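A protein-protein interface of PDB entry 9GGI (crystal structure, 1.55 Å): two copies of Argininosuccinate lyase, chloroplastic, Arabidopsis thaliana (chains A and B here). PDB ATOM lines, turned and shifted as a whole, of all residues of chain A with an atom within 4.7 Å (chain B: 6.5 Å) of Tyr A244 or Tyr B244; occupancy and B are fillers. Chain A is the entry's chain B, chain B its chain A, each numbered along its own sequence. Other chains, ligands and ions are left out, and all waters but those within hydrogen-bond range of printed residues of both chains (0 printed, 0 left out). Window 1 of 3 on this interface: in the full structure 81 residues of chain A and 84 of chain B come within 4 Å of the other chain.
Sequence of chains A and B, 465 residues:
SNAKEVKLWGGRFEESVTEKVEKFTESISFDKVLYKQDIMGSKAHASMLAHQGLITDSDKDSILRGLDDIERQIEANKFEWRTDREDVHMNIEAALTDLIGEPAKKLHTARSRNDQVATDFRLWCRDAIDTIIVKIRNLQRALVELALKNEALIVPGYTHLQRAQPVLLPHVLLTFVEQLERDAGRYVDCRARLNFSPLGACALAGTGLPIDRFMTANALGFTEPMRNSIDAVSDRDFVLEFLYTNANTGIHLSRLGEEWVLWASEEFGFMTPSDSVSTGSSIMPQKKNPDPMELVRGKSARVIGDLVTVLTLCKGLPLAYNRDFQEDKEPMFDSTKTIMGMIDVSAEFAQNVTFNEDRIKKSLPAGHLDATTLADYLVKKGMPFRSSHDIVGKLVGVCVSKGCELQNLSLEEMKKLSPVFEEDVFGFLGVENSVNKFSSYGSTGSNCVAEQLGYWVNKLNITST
The side-chain carboxylate (OD2) of Asp A237 is in salt-bridge range of the guanidinium group (NH2) of Arg B186 (3.0 Å). The guanidinium group (NH1) of Arg B186 lies within salt-bridge range of the side-chain carboxylate (OE1) of Glu A241 (3.0 Å). OD2 of Asp B237 lies within salt-bridge range of NH2 of Arg A186 (3.0 Å). The side-chain amide oxygen (OD1) of Asn A248 sits close to the side-chain carboxylate (OD1) of Asp B237 (3.0 Å). The guanidinium group of Arg A186 lies within salt-bridge range of the side-chain carboxylate of Glu B241 (3.0 Å). The side-chain hydroxyl (OH) of Tyr A244 sits close to the backbone NH (N) of Glu B241. OH of Tyr B244 sits close to N of Glu A241, 3.2 Å away. OD1 of Asp A237 sits close to OD1 of Asn B248 (3.1 Å).
The backbone carbonyl oxygen (O) of Glu B241 lies within hydrogen-bond range of the side-chain hydroxyl (OG1) of Thr B245 (2.8 Å). The side-chain hydroxyl (OH) of Tyr B244 is in hydrogen-bond range of the side-chain amide nitrogen (ND2) of Asn B248, 2.7 Å away. The backbone carbonyl oxygen (O) of Glu A241 sits at hydrogen-bond distance from the side-chain hydroxyl (OG1) of Thr A245, at 2.8 Å. OH of Tyr A244 is in hydrogen-bond range of ND2 of Asn A248 (2.7 Å).
Among the printed residues, merely in contact across the chains: Leu A240 with Tyr B244 (3.7 Å), Leu A240 with Asn B248 (3.5 Å), Tyr A244 with Leu B240 (3.8 Å), Tyr A244 with Tyr B244 (3.4 Å), Asn A248 with Leu B240 (3.6 Å) and Leu A307 with Leu B311 (3.9 Å).
Printed residues of chain B within 4 Å of Asp A237: Arg B186 and Asn B248. Of the printed residues of chain B, Glu A241 touches Arg B186 (3.0 Å) and Tyr B244 (3.2 Å). Leu A243 touches none of the printed residues of chain B. Tyr A244 touches just these residues of chain B: Leu B240 (3.8 Å), Glu B241 (3.2 Å) and Tyr B244 (3.4 Å). Printed residues of chain A within 4 Å of Tyr B244: Leu A240 (3.7 Å), Glu A241 (3.2 Å) and Tyr A244 (3.4 Å). Val B303 touches none of the printed residues of chain A. The nearest printed residue of chain A that does not touch Leu B311 is Ala A247 (4.5 Å).
Of the 12 printed residues of chain A, 7 touch a printed residue of chain B. Hydrophobic or aromatic side chains of chain A that line the printed part of chain B: Leu A240, Tyr A244 and Leu A307. Among the printed residues, 14 pairs touch across the chains.
Arg A186 touches Asp B237, and with the chains exchanged Asp A237 touches Arg B186. Arg A186 touches Glu B241, and with the chains exchanged Glu A241 touches Arg B186. Asp A237 touches Asn B248, and with the chains exchanged Asn A248 touches Asp B237. Tyr A244 touches its own counterpart, Tyr B244. Positions printed for both chains: 186, 237, 240, 241, 242, 243, 244, 245, 246, 247, 248 and 307. Of the 14 pairs that touch across the chains among the printed residues, 13 have their exchanged pair printed and touching as well.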
ATOM      1  N   ARG A 186      23.084 -10.232  30.341  1.00  0.00           N
ATOM      2  CA  ARG A 186      24.435 -10.467  29.825  1.00  0.00           C
ATOM      3  C   ARG A 186      25.433  -9.454  30.396  1.00  0.00           C
ATOM      4  O   ARG A 186      26.543  -9.847  30.729  1.00  0.00           O
ATOM      5  CB  ARG A 186      24.439 -10.445  28.297  1.00  0.00           C
ATOM      6  CG  ARG A 186      24.050 -11.798  27.713  1.00  0.00           C
ATOM      7  CD  ARG A 186      24.174 -11.810  26.204  1.00  0.00           C
ATOM      8  NE  ARG A 186      23.027 -11.168  25.552  1.00  0.00           N
ATOM      9  CZ  ARG A 186      21.861 -11.734  25.238  1.00  0.00           C
ATOM     10  NH1 ARG A 186      21.713 -13.051  25.359  1.00  0.00           N
ATOM     11  NH2 ARG A 186      20.927 -11.003  24.705  1.00  0.00           N
ATOM     12  N   ASP A 237      39.535 -11.776  27.939  1.00  0.00           N
ATOM     13  CA  ASP A 237      38.175 -12.310  27.765  1.00  0.00           C
ATOM     14  C   ASP A 237      37.127 -11.266  28.115  1.00  0.00           C
ATOM     15  O   ASP A 237      36.055 -11.226  27.543  1.00  0.00           O
ATOM     16  CB  ASP A 237      37.895 -13.535  28.604  1.00  0.00           C
ATOM     17  CG  ASP A 237      38.659 -14.780  28.218  1.00  0.00           C
ATOM     18  OD1 ASP A 237      39.379 -14.760  27.199  1.00  0.00           O
ATOM     19  OD2 ASP A 237      38.522 -15.779  28.975  1.00  0.00           O
ATOM     20  N   LEU A 240      36.344  -9.286  25.116  1.00  0.00           N
ATOM     21  CA  LEU A 240      35.551 -10.043  24.159  1.00  0.00           C
ATOM     22  C   LEU A 240      34.086 -10.201  24.578  1.00  0.00           C
ATOM     23  O   LEU A 240      33.177 -10.014  23.776  1.00  0.00           O
ATOM     24  CB  LEU A 240      36.143 -11.450  24.013  1.00  0.00           C
ATOM     25  CG  LEU A 240      37.505 -11.503  23.340  1.00  0.00           C
ATOM     26  CD1 LEU A 240      38.096 -12.890  23.409  1.00  0.00           C
ATOM     27  CD2 LEU A 240      37.465 -10.932  21.942  1.00  0.00           C
ATOM     28  N   GLU A 241      33.865 -10.496  25.856  1.00  0.00           N
ATOM     29  CA  GLU A 241      32.524 -10.732  26.338  1.00  0.00           C
ATOM     30  C   GLU A 241      31.715  -9.426  26.317  1.00  0.00           C
ATOM     31  O   GLU A 241      30.546  -9.436  26.005  1.00  0.00           O
ATOM     32  CB  GLU A 241      32.524 -11.394  27.731  1.00  0.00           C
ATOM     33  CG  GLU A 241      31.151 -11.870  28.223  1.00  0.00           C
ATOM     34  CD  GLU A 241      31.193 -12.612  29.557  1.00  0.00           C
ATOM     35  OE1 GLU A 241      32.287 -13.068  30.000  1.00  0.00           O
ATOM     36  OE2 GLU A 241      30.062 -12.775  30.116  1.00  0.00           O
ATOM     37  N   PHE A 242      32.348  -8.314  26.701  1.00  0.00           N
ATOM     38  CA  PHE A 242      31.689  -7.007  26.676  1.00  0.00           C
ATOM     39  C   PHE A 242      31.370  -6.634  25.217  1.00  0.00           C
ATOM     40  O   PHE A 242      30.301  -6.150  24.917  1.00  0.00           O
ATOM     41  CB  PHE A 242      32.629  -6.045  27.440  1.00  0.00           C
ATOM     42  CG  PHE A 242      32.121  -4.633  27.680  1.00  0.00           C
ATOM     43  CD1 PHE A 242      30.833  -4.235  27.404  1.00  0.00           C
ATOM     44  CD2 PHE A 242      32.991  -3.692  28.234  1.00  0.00           C
ATOM     45  CE1 PHE A 242      30.401  -2.937  27.584  1.00  0.00           C
ATOM     46  CE2 PHE A 242      32.564  -2.372  28.408  1.00  0.00           C
ATOM     47  CZ  PHE A 242      31.261  -2.013  28.134  1.00  0.00           C
ATOM     48  N   LEU A 243      32.334  -6.841  24.313  1.00  0.00           N
ATOM     49  CA  LEU A 243      32.078  -6.562  22.903  1.00  0.00           C
ATOM     50  C   LEU A 243      30.891  -7.361  22.366  1.00  0.00           C
ATOM     51  O   LEU A 243      30.109  -6.858  21.607  1.00  0.00           O
ATOM     52  CB  LEU A 243      33.341  -6.869  22.090  1.00  0.00           C
ATOM     53  CG  LEU A 243      34.526  -5.893  22.256  1.00  0.00           C
ATOM     54  CD1 LEU A 243      35.792  -6.459  21.723  1.00  0.00           C
ATOM     55  CD2 LEU A 243      34.229  -4.549  21.590  1.00  0.00           C
ATOM     56  N   TYR A 244      30.856  -8.655  22.697  1.00  0.00           N
ATOM     57  CA  TYR A 244      29.763  -9.494  22.215  1.00  0.00           C
ATOM     58  C   TYR A 244      28.423  -9.017  22.808  1.00  0.00           C
ATOM     59  O   TYR A 244      27.425  -8.883  22.103  1.00  0.00           O
ATOM     60  CB  TYR A 244      29.993 -10.993  22.518  1.00  0.00           C
ATOM     61  CG  TYR A 244      28.635 -11.707  22.525  1.00  0.00           C
ATOM     62  CD1 TYR A 244      27.889 -11.877  21.378  1.00  0.00           C
ATOM     63  CD2 TYR A 244      28.075 -12.066  23.721  1.00  0.00           C
ATOM     64  CE1 TYR A 244      26.618 -12.397  21.443  1.00  0.00           C
ATOM     65  CE2 TYR A 244      26.807 -12.596  23.793  1.00  0.00           C
ATOM     66  CZ  TYR A 244      26.066 -12.719  22.656  1.00  0.00           C
ATOM     67  OH  TYR A 244      24.776 -13.198  22.916  1.00  0.00           O
ATOM     68  N   THR A 245      28.447  -8.666  24.107  1.00  0.00           N
ATOM     69  CA  THR A 245      27.210  -8.239  24.735  1.00  0.00           C
ATOM     70  C   THR A 245      26.703  -6.955  24.063  1.00  0.00           C
ATOM     71  O   THR A 245      25.531  -6.784  23.764  1.00  0.00           O
ATOM     72  CB  THR A 245      27.451  -8.031  26.235  1.00  0.00           C
ATOM     73  OG1 THR A 245      27.824  -9.289  26.805  1.00  0.00           O
ATOM     74  CG2 THR A 245      26.165  -7.629  26.945  1.00  0.00           C
ATOM     75  N   ASN A 246      27.632  -6.026  23.765  1.00  0.00           N
ATOM     76  CA  ASN A 246      27.258  -4.857  22.994  1.00  0.00           C
ATOM     77  C   ASN A 246      26.702  -5.236  21.615  1.00  0.00           C
ATOM     78  O   ASN A 246      25.762  -4.610  21.161  1.00  0.00           O
ATOM     79  CB  ASN A 246      28.394  -3.824  22.822  1.00  0.00           C
ATOM     80  CG  ASN A 246      28.859  -3.193  24.109  1.00  0.00           C
ATOM     81  OD1 ASN A 246      28.142  -3.190  25.108  1.00  0.00           O
ATOM     82  ND2 ASN A 246      30.014  -2.550  24.052  1.00  0.00           N
ATOM     83  N   ALA A 247      27.370  -6.188  20.933  1.00  0.00           N
ATOM     84  CA  ALA A 247      26.887  -6.562  19.616  1.00  0.00           C
ATOM     85  C   ALA A 247      25.474  -7.133  19.635  1.00  0.00           C
ATOM     86  O   ALA A 247      24.676  -6.861  18.726  1.00  0.00           O
ATOM     87  CB  ALA A 247      27.886  -7.514  18.965  1.00  0.00           C
ATOM     88  N   ASN A 248      25.168  -7.954  20.636  1.00  0.00           N
ATOM     89  CA  ASN A 248      23.817  -8.515  20.675  1.00  0.00           C
ATOM     90  C   ASN A 248      22.796  -7.419  20.996  1.00  0.00           C
ATOM     91  O   ASN A 248      21.671  -7.416  20.476  1.00  0.00           O
ATOM     92  CB  ASN A 248      23.729  -9.734  21.588  1.00  0.00           C
ATOM     93  CG  ASN A 248      22.546 -10.664  21.337  1.00  0.00           C
ATOM     94  OD1 ASN A 248      21.468 -10.295  20.828  1.00  0.00           O
ATOM     95  ND2 ASN A 248      22.775 -11.904  21.654  1.00  0.00           N
ATOM     96  N   LEU A 307      33.763  -6.288  17.660  1.00  0.00           N
ATOM     97  CA  LEU A 307      33.897  -7.634  18.182  1.00  0.00           C
ATOM     98  C   LEU A 307      34.843  -8.509  17.332  1.00  0.00           C
ATOM     99  O   LEU A 307      35.705  -9.179  17.855  1.00  0.00           O
ATOM    100  CB  LEU A 307      32.494  -8.271  18.281  1.00  0.00           C
ATOM    101  CG  LEU A 307      32.497  -9.762  18.614  1.00  0.00           C
ATOM    102  CD1 LEU A 307      33.062 -10.077  19.987  1.00  0.00           C
ATOM    103  CD2 LEU A 307      31.061 -10.263  18.482  1.00  0.00           C
ATOM    104  N   ARG B 186      30.783 -19.014  31.233  1.00  0.00           N
ATOM    105  CA  ARG B 186      29.957 -18.471  30.172  1.00  0.00           C
ATOM    106  C   ARG B 186      28.932 -19.508  29.685  1.00  0.00           C
ATOM    107  O   ARG B 186      27.804 -19.151  29.404  1.00  0.00           O
ATOM    108  CB  ARG B 186      30.812 -17.976  28.992  1.00  0.00           C
ATOM    109  CG  ARG B 186      31.446 -16.621  29.233  1.00  0.00           C
ATOM    110  CD  ARG B 186      32.209 -16.037  28.093  1.00  0.00           C
ATOM    111  NE  ARG B 186      33.539 -16.608  27.999  1.00  0.00           N
ATOM    112  CZ  ARG B 186      34.600 -16.117  28.630  1.00  0.00           C
ATOM    113  NH1 ARG B 186      34.488 -14.997  29.313  1.00  0.00           N
ATOM    114  NH2 ARG B 186      35.751 -16.774  28.554  1.00  0.00           N
ATOM    115  N   ASP B 237      18.782 -15.097  20.409  1.00  0.00           N
ATOM    116  CA  ASP B 237      19.924 -14.699  21.205  1.00  0.00           C
ATOM    117  C   ASP B 237      20.670 -15.877  21.778  1.00  0.00           C
ATOM    118  O   ASP B 237      21.896 -15.842  21.969  1.00  0.00           O
ATOM    119  CB  ASP B 237      19.518 -13.846  22.394  1.00  0.00           C
ATOM    120  CG  ASP B 237      18.978 -12.466  22.067  1.00  0.00           C
ATOM    121  OD1 ASP B 237      19.012 -12.075  20.867  1.00  0.00           O
ATOM    122  OD2 ASP B 237      18.535 -11.781  23.061  1.00  0.00           O
ATOM    123  N   PHE B 238      19.962 -16.924  22.119  1.00  0.00           N
ATOM    124  CA  PHE B 238      20.599 -18.123  22.681  1.00  0.00           C
ATOM    125  C   PHE B 238      21.631 -18.687  21.702  1.00  0.00           C
ATOM    126  O   PHE B 238      22.631 -19.228  22.131  1.00  0.00           O
ATOM    127  CB  PHE B 238      19.583 -19.189  23.127  1.00  0.00           C
ATOM    128  CG  PHE B 238      18.681 -19.769  22.037  1.00  0.00           C
ATOM    129  CD1 PHE B 238      17.560 -19.092  21.587  1.00  0.00           C
ATOM    130  CD2 PHE B 238      19.008 -20.957  21.388  1.00  0.00           C
ATOM    131  CE1 PHE B 238      16.767 -19.606  20.560  1.00  0.00           C
ATOM    132  CE2 PHE B 238      18.206 -21.466  20.356  1.00  0.00           C
ATOM    133  CZ  PHE B 238      17.081 -20.792  19.970  1.00  0.00           C
ATOM    134  N   VAL B 239      21.300 -18.640  20.382  1.00  0.00           N
ATOM    135  CA  VAL B 239      22.247 -19.087  19.379  1.00  0.00           C
ATOM    136  C   VAL B 239      23.472 -18.164  19.355  1.00  0.00           C
ATOM    137  O   VAL B 239      24.597 -18.619  19.370  1.00  0.00           O
ATOM    138  CB  VAL B 239      21.545 -19.097  18.003  1.00  0.00           C
ATOM    139  CG1 VAL B 239      22.455 -19.680  16.931  1.00  0.00           C
ATOM    140  CG2 VAL B 239      20.238 -19.875  18.031  1.00  0.00           C
ATOM    141  N   LEU B 240      23.223 -16.863  19.347  1.00  0.00           N
ATOM    142  CA  LEU B 240      24.322 -15.917  19.340  1.00  0.00           C
ATOM    143  C   LEU B 240      25.247 -16.071  20.537  1.00  0.00           C
ATOM    144  O   LEU B 240      26.488 -16.073  20.414  1.00  0.00           O
ATOM    145  CB  LEU B 240      23.817 -14.476  19.289  1.00  0.00           C
ATOM    146  CG  LEU B 240      23.036 -14.087  18.024  1.00  0.00           C
ATOM    147  CD1 LEU B 240      22.381 -12.693  18.121  1.00  0.00           C
ATOM    148  CD2 LEU B 240      23.956 -14.153  16.835  1.00  0.00           C
ATOM    149  N   GLU B 241      24.637 -16.175  21.725  1.00  0.00           N
ATOM    150  CA  GLU B 241      25.441 -16.299  22.938  1.00  0.00           C
ATOM    151  C   GLU B 241      26.249 -17.610  22.978  1.00  0.00           C
ATOM    152  O   GLU B 241      27.414 -17.608  23.408  1.00  0.00           O
ATOM    153  CB  GLU B 241      24.560 -16.126  24.163  1.00  0.00           C
ATOM    154  CG  GLU B 241      25.357 -16.019  25.466  1.00  0.00           C
ATOM    155  CD  GLU B 241      24.500 -15.676  26.657  1.00  0.00           C
ATOM    156  OE1 GLU B 241      23.310 -15.321  26.566  1.00  0.00           O
ATOM    157  OE2 GLU B 241      25.035 -15.857  27.811  1.00  0.00           O
ATOM    158  N   PHE B 242      25.661 -18.706  22.491  1.00  0.00           N
ATOM    159  CA  PHE B 242      26.360 -19.980  22.461  1.00  0.00           C
ATOM    160  C   PHE B 242      27.490 -19.912  21.410  1.00  0.00           C
ATOM    161  O   PHE B 242      28.577 -20.343  21.662  1.00  0.00           O
ATOM    162  CB  PHE B 242      25.261 -21.034  22.158  1.00  0.00           C
ATOM    163  CG  PHE B 242      25.680 -22.494  22.181  1.00  0.00           C
ATOM    164  CD1 PHE B 242      26.918 -22.923  22.576  1.00  0.00           C
ATOM    165  CD2 PHE B 242      24.766 -23.451  21.780  1.00  0.00           C
ATOM    166  CE1 PHE B 242      27.295 -24.261  22.571  1.00  0.00           C
ATOM    167  CE2 PHE B 242      25.121 -24.797  21.763  1.00  0.00           C
ATOM    168  CZ  PHE B 242      26.360 -25.221  22.181  1.00  0.00           C
ATOM    169  N   LEU B 243      27.204 -19.348  20.240  1.00  0.00           N
ATOM    170  CA  LEU B 243      28.256 -19.130  19.243  1.00  0.00           C
ATOM    171  C   LEU B 243      29.440 -18.319  19.784  1.00  0.00           C
ATOM    172  O   LEU B 243      30.587 -18.664  19.517  1.00  0.00           O
ATOM    173  CB  LEU B 243      27.671 -18.451  18.005  1.00  0.00           C
ATOM    174  CG  LEU B 243      26.745 -19.304  17.131  1.00  0.00           C
ATOM    175  CD1 LEU B 243      25.979 -18.429  16.198  1.00  0.00           C
ATOM    176  CD2 LEU B 243      27.533 -20.356  16.379  1.00  0.00           C
ATOM    177  N   TYR B 244      29.127 -17.242  20.496  1.00  0.00           N
ATOM    178  CA  TYR B 244      30.182 -16.392  21.034  1.00  0.00           C
ATOM    179  C   TYR B 244      30.969 -17.194  22.075  1.00  0.00           C
ATOM    180  O   TYR B 244      32.177 -17.191  22.121  1.00  0.00           O
ATOM    181  CB  TYR B 244      29.676 -15.040  21.626  1.00  0.00           C
ATOM    182  CG  TYR B 244      30.673 -14.536  22.676  1.00  0.00           C
ATOM    183  CD1 TYR B 244      31.929 -14.086  22.298  1.00  0.00           C
ATOM    184  CD2 TYR B 244      30.352 -14.623  24.006  1.00  0.00           C
ATOM    185  CE1 TYR B 244      32.859 -13.801  23.286  1.00  0.00           C
ATOM    186  CE2 TYR B 244      31.281 -14.352  24.981  1.00  0.00           C
ATOM    187  CZ  TYR B 244      32.512 -13.931  24.616  1.00  0.00           C
ATOM    188  OH  TYR B 244      33.418 -13.707  25.673  1.00  0.00           O
ATOM    189  N   THR B 245      30.239 -17.907  22.973  1.00  0.00           N
ATOM    190  CA  THR B 245      30.935 -18.657  24.007  1.00  0.00           C
ATOM    191  C   THR B 245      31.854 -19.738  23.375  1.00  0.00           C
ATOM    192  O   THR B 245      32.992 -19.932  23.789  1.00  0.00           O
ATOM    193  CB  THR B 245      29.914 -19.289  24.975  1.00  0.00           C
ATOM    194  OG1 THR B 245      29.125 -18.255  25.591  1.00  0.00           O
ATOM    195  CG2 THR B 245      30.631 -20.054  26.084  1.00  0.00           C
ATOM    196  N   ASN B 246      31.396 -20.355  22.288  1.00  0.00           N
ATOM    197  CA  ASN B 246      32.273 -21.306  21.597  1.00  0.00           C
ATOM    198  C   ASN B 246      33.483 -20.561  21.006  1.00  0.00           C
ATOM    199  O   ASN B 246      34.558 -21.082  21.018  1.00  0.00           O
ATOM    200  CB  ASN B 246      31.515 -22.013  20.471  1.00  0.00           C
ATOM    201  CG  ASN B 246      30.511 -23.046  20.954  1.00  0.00           C
ATOM    202  OD1 ASN B 246      30.456 -23.414  22.136  1.00  0.00           O
ATOM    203  ND2 ASN B 246      29.656 -23.512  20.036  1.00  0.00           N
ATOM    204  N   ALA B 247      33.236 -19.383  20.434  1.00  0.00           N
ATOM    205  CA  ALA B 247      34.351 -18.616  19.859  1.00  0.00           C
ATOM    206  C   ALA B 247      35.435 -18.212  20.862  1.00  0.00           C
ATOM    207  O   ALA B 247      36.629 -18.321  20.548  1.00  0.00           O
ATOM    208  CB  ALA B 247      33.817 -17.406  19.062  1.00  0.00           C
ATOM    209  N   ASN B 248      35.038 -17.805  22.071  1.00  0.00           N
ATOM    210  CA  ASN B 248      36.009 -17.478  23.106  1.00  0.00           C
ATOM    211  C   ASN B 248      36.768 -18.729  23.539  1.00  0.00           C
ATOM    212  O   ASN B 248      37.964 -18.706  23.805  1.00  0.00           O
ATOM    213  CB  ASN B 248      35.374 -16.664  24.218  1.00  0.00           C
ATOM    214  CG  ASN B 248      36.371 -15.845  25.016  1.00  0.00           C
ATOM    215  OD1 ASN B 248      37.598 -16.149  25.073  1.00  0.00           O
ATOM    216  ND2 ASN B 248      35.911 -14.721  25.456  1.00  0.00           N
ATOM    217  N   THR B 249      36.060 -19.866  23.677  1.00  0.00           N
ATOM    218  CA  THR B 249      36.730 -21.105  24.010  1.00  0.00           C
ATOM    219  C   THR B 249      37.778 -21.445  22.953  1.00  0.00           C
ATOM    220  O   THR B 249      38.870 -21.867  23.219  1.00  0.00           O
ATOM    221  CB  THR B 249      35.715 -22.240  24.197  1.00  0.00           C
ATOM    222  OG1 THR B 249      34.711 -21.833  25.135  1.00  0.00           O
ATOM    223  CG2 THR B 249      36.371 -23.536  24.671  1.00  0.00           C
ATOM    224  N   VAL B 303      34.956 -21.226  13.861  1.00  0.00           N
ATOM    225  CA  VAL B 303      34.072 -20.913  14.995  1.00  0.00           C
ATOM    226  C   VAL B 303      33.752 -19.405  15.055  1.00  0.00           C
ATOM    227  O   VAL B 303      32.620 -18.997  15.314  1.00  0.00           O
ATOM    228  CB  VAL B 303      34.690 -21.475  16.298  1.00  0.00           C
ATOM    229  CG1 VAL B 303      33.779 -21.211  17.494  1.00  0.00           C
ATOM    230  CG2 VAL B 303      34.927 -22.983  16.221  1.00  0.00           C
ATOM    231  N   LEU B 307      29.971 -17.511  14.220  1.00  0.00           N
ATOM    232  CA  LEU B 307      29.383 -16.406  14.994  1.00  0.00           C
ATOM    233  C   LEU B 307      29.024 -15.219  14.093  1.00  0.00           C
ATOM    234  O   LEU B 307      27.942 -14.682  14.186  1.00  0.00           O
ATOM    235  CB  LEU B 307      30.386 -15.991  16.079  1.00  0.00           C
ATOM    236  CG  LEU B 307      30.030 -14.736  16.872  1.00  0.00           C
ATOM    237  CD1 LEU B 307      28.775 -14.803  17.665  1.00  0.00           C
ATOM    238  CD2 LEU B 307      31.217 -14.357  17.745  1.00  0.00           C
ATOM    239  N   LEU B 311      25.288 -13.376  13.601  1.00  0.00           N
ATOM    240  CA  LEU B 311      25.162 -11.952  13.858  1.00  0.00           C
ATOM    241  C   LEU B 311      24.616 -11.200  12.656  1.00  0.00           C
ATOM    242  O   LEU B 311      23.698 -10.386  12.777  1.00  0.00           O
ATOM    243  CB  LEU B 311      26.466 -11.316  14.293  1.00  0.00           C
ATOM    244  CG  LEU B 311      27.021 -11.708  15.653  1.00  0.00           C
ATOM    245  CD1 LEU B 311      28.478 -11.395  15.824  1.00  0.00           C
ATOM    246  CD2 LEU B 311      26.200 -11.036  16.765  1.00  0.00           C
ATOM    247  N   MET B 332      25.414 -23.151  13.994  1.00  0.00           N
ATOM    248  CA  MET B 332      25.451 -23.594  15.390  1.00  0.00           C
ATOM    249  C   MET B 332      25.955 -25.031  15.492  1.00  0.00           C
ATOM    250  O   MET B 332      26.746 -25.414  16.331  1.00  0.00           O
ATOM    251  CB  MET B 332      24.064 -23.466  16.044  1.00  0.00           C
ATOM    252  CG  MET B 332      24.018 -23.647  17.548  1.00  0.00           C
ATOM    253  SD  MET B 332      24.824 -22.246  18.393  1.00  0.00           S
ATOM    254  CE  MET B 332      26.449 -22.888  18.840  1.00  0.00           C
ATOM    255  N   SER B 335      29.724 -24.999  14.698  1.00  0.00           N
ATOM    256  CA  SER B 335      30.495 -24.404  15.785  1.00  0.00           C
ATOM    257  C   SER B 335      30.639 -25.385  16.939  1.00  0.00           C
ATOM    258  O   SER B 335      31.708 -25.549  17.513  1.00  0.00           O
ATOM    259  CB  SER B 335      29.770 -23.154  16.248  1.00  0.00           C
ATOM    260  OG  SER B 335      30.431 -22.548  17.382  1.00  0.00           O
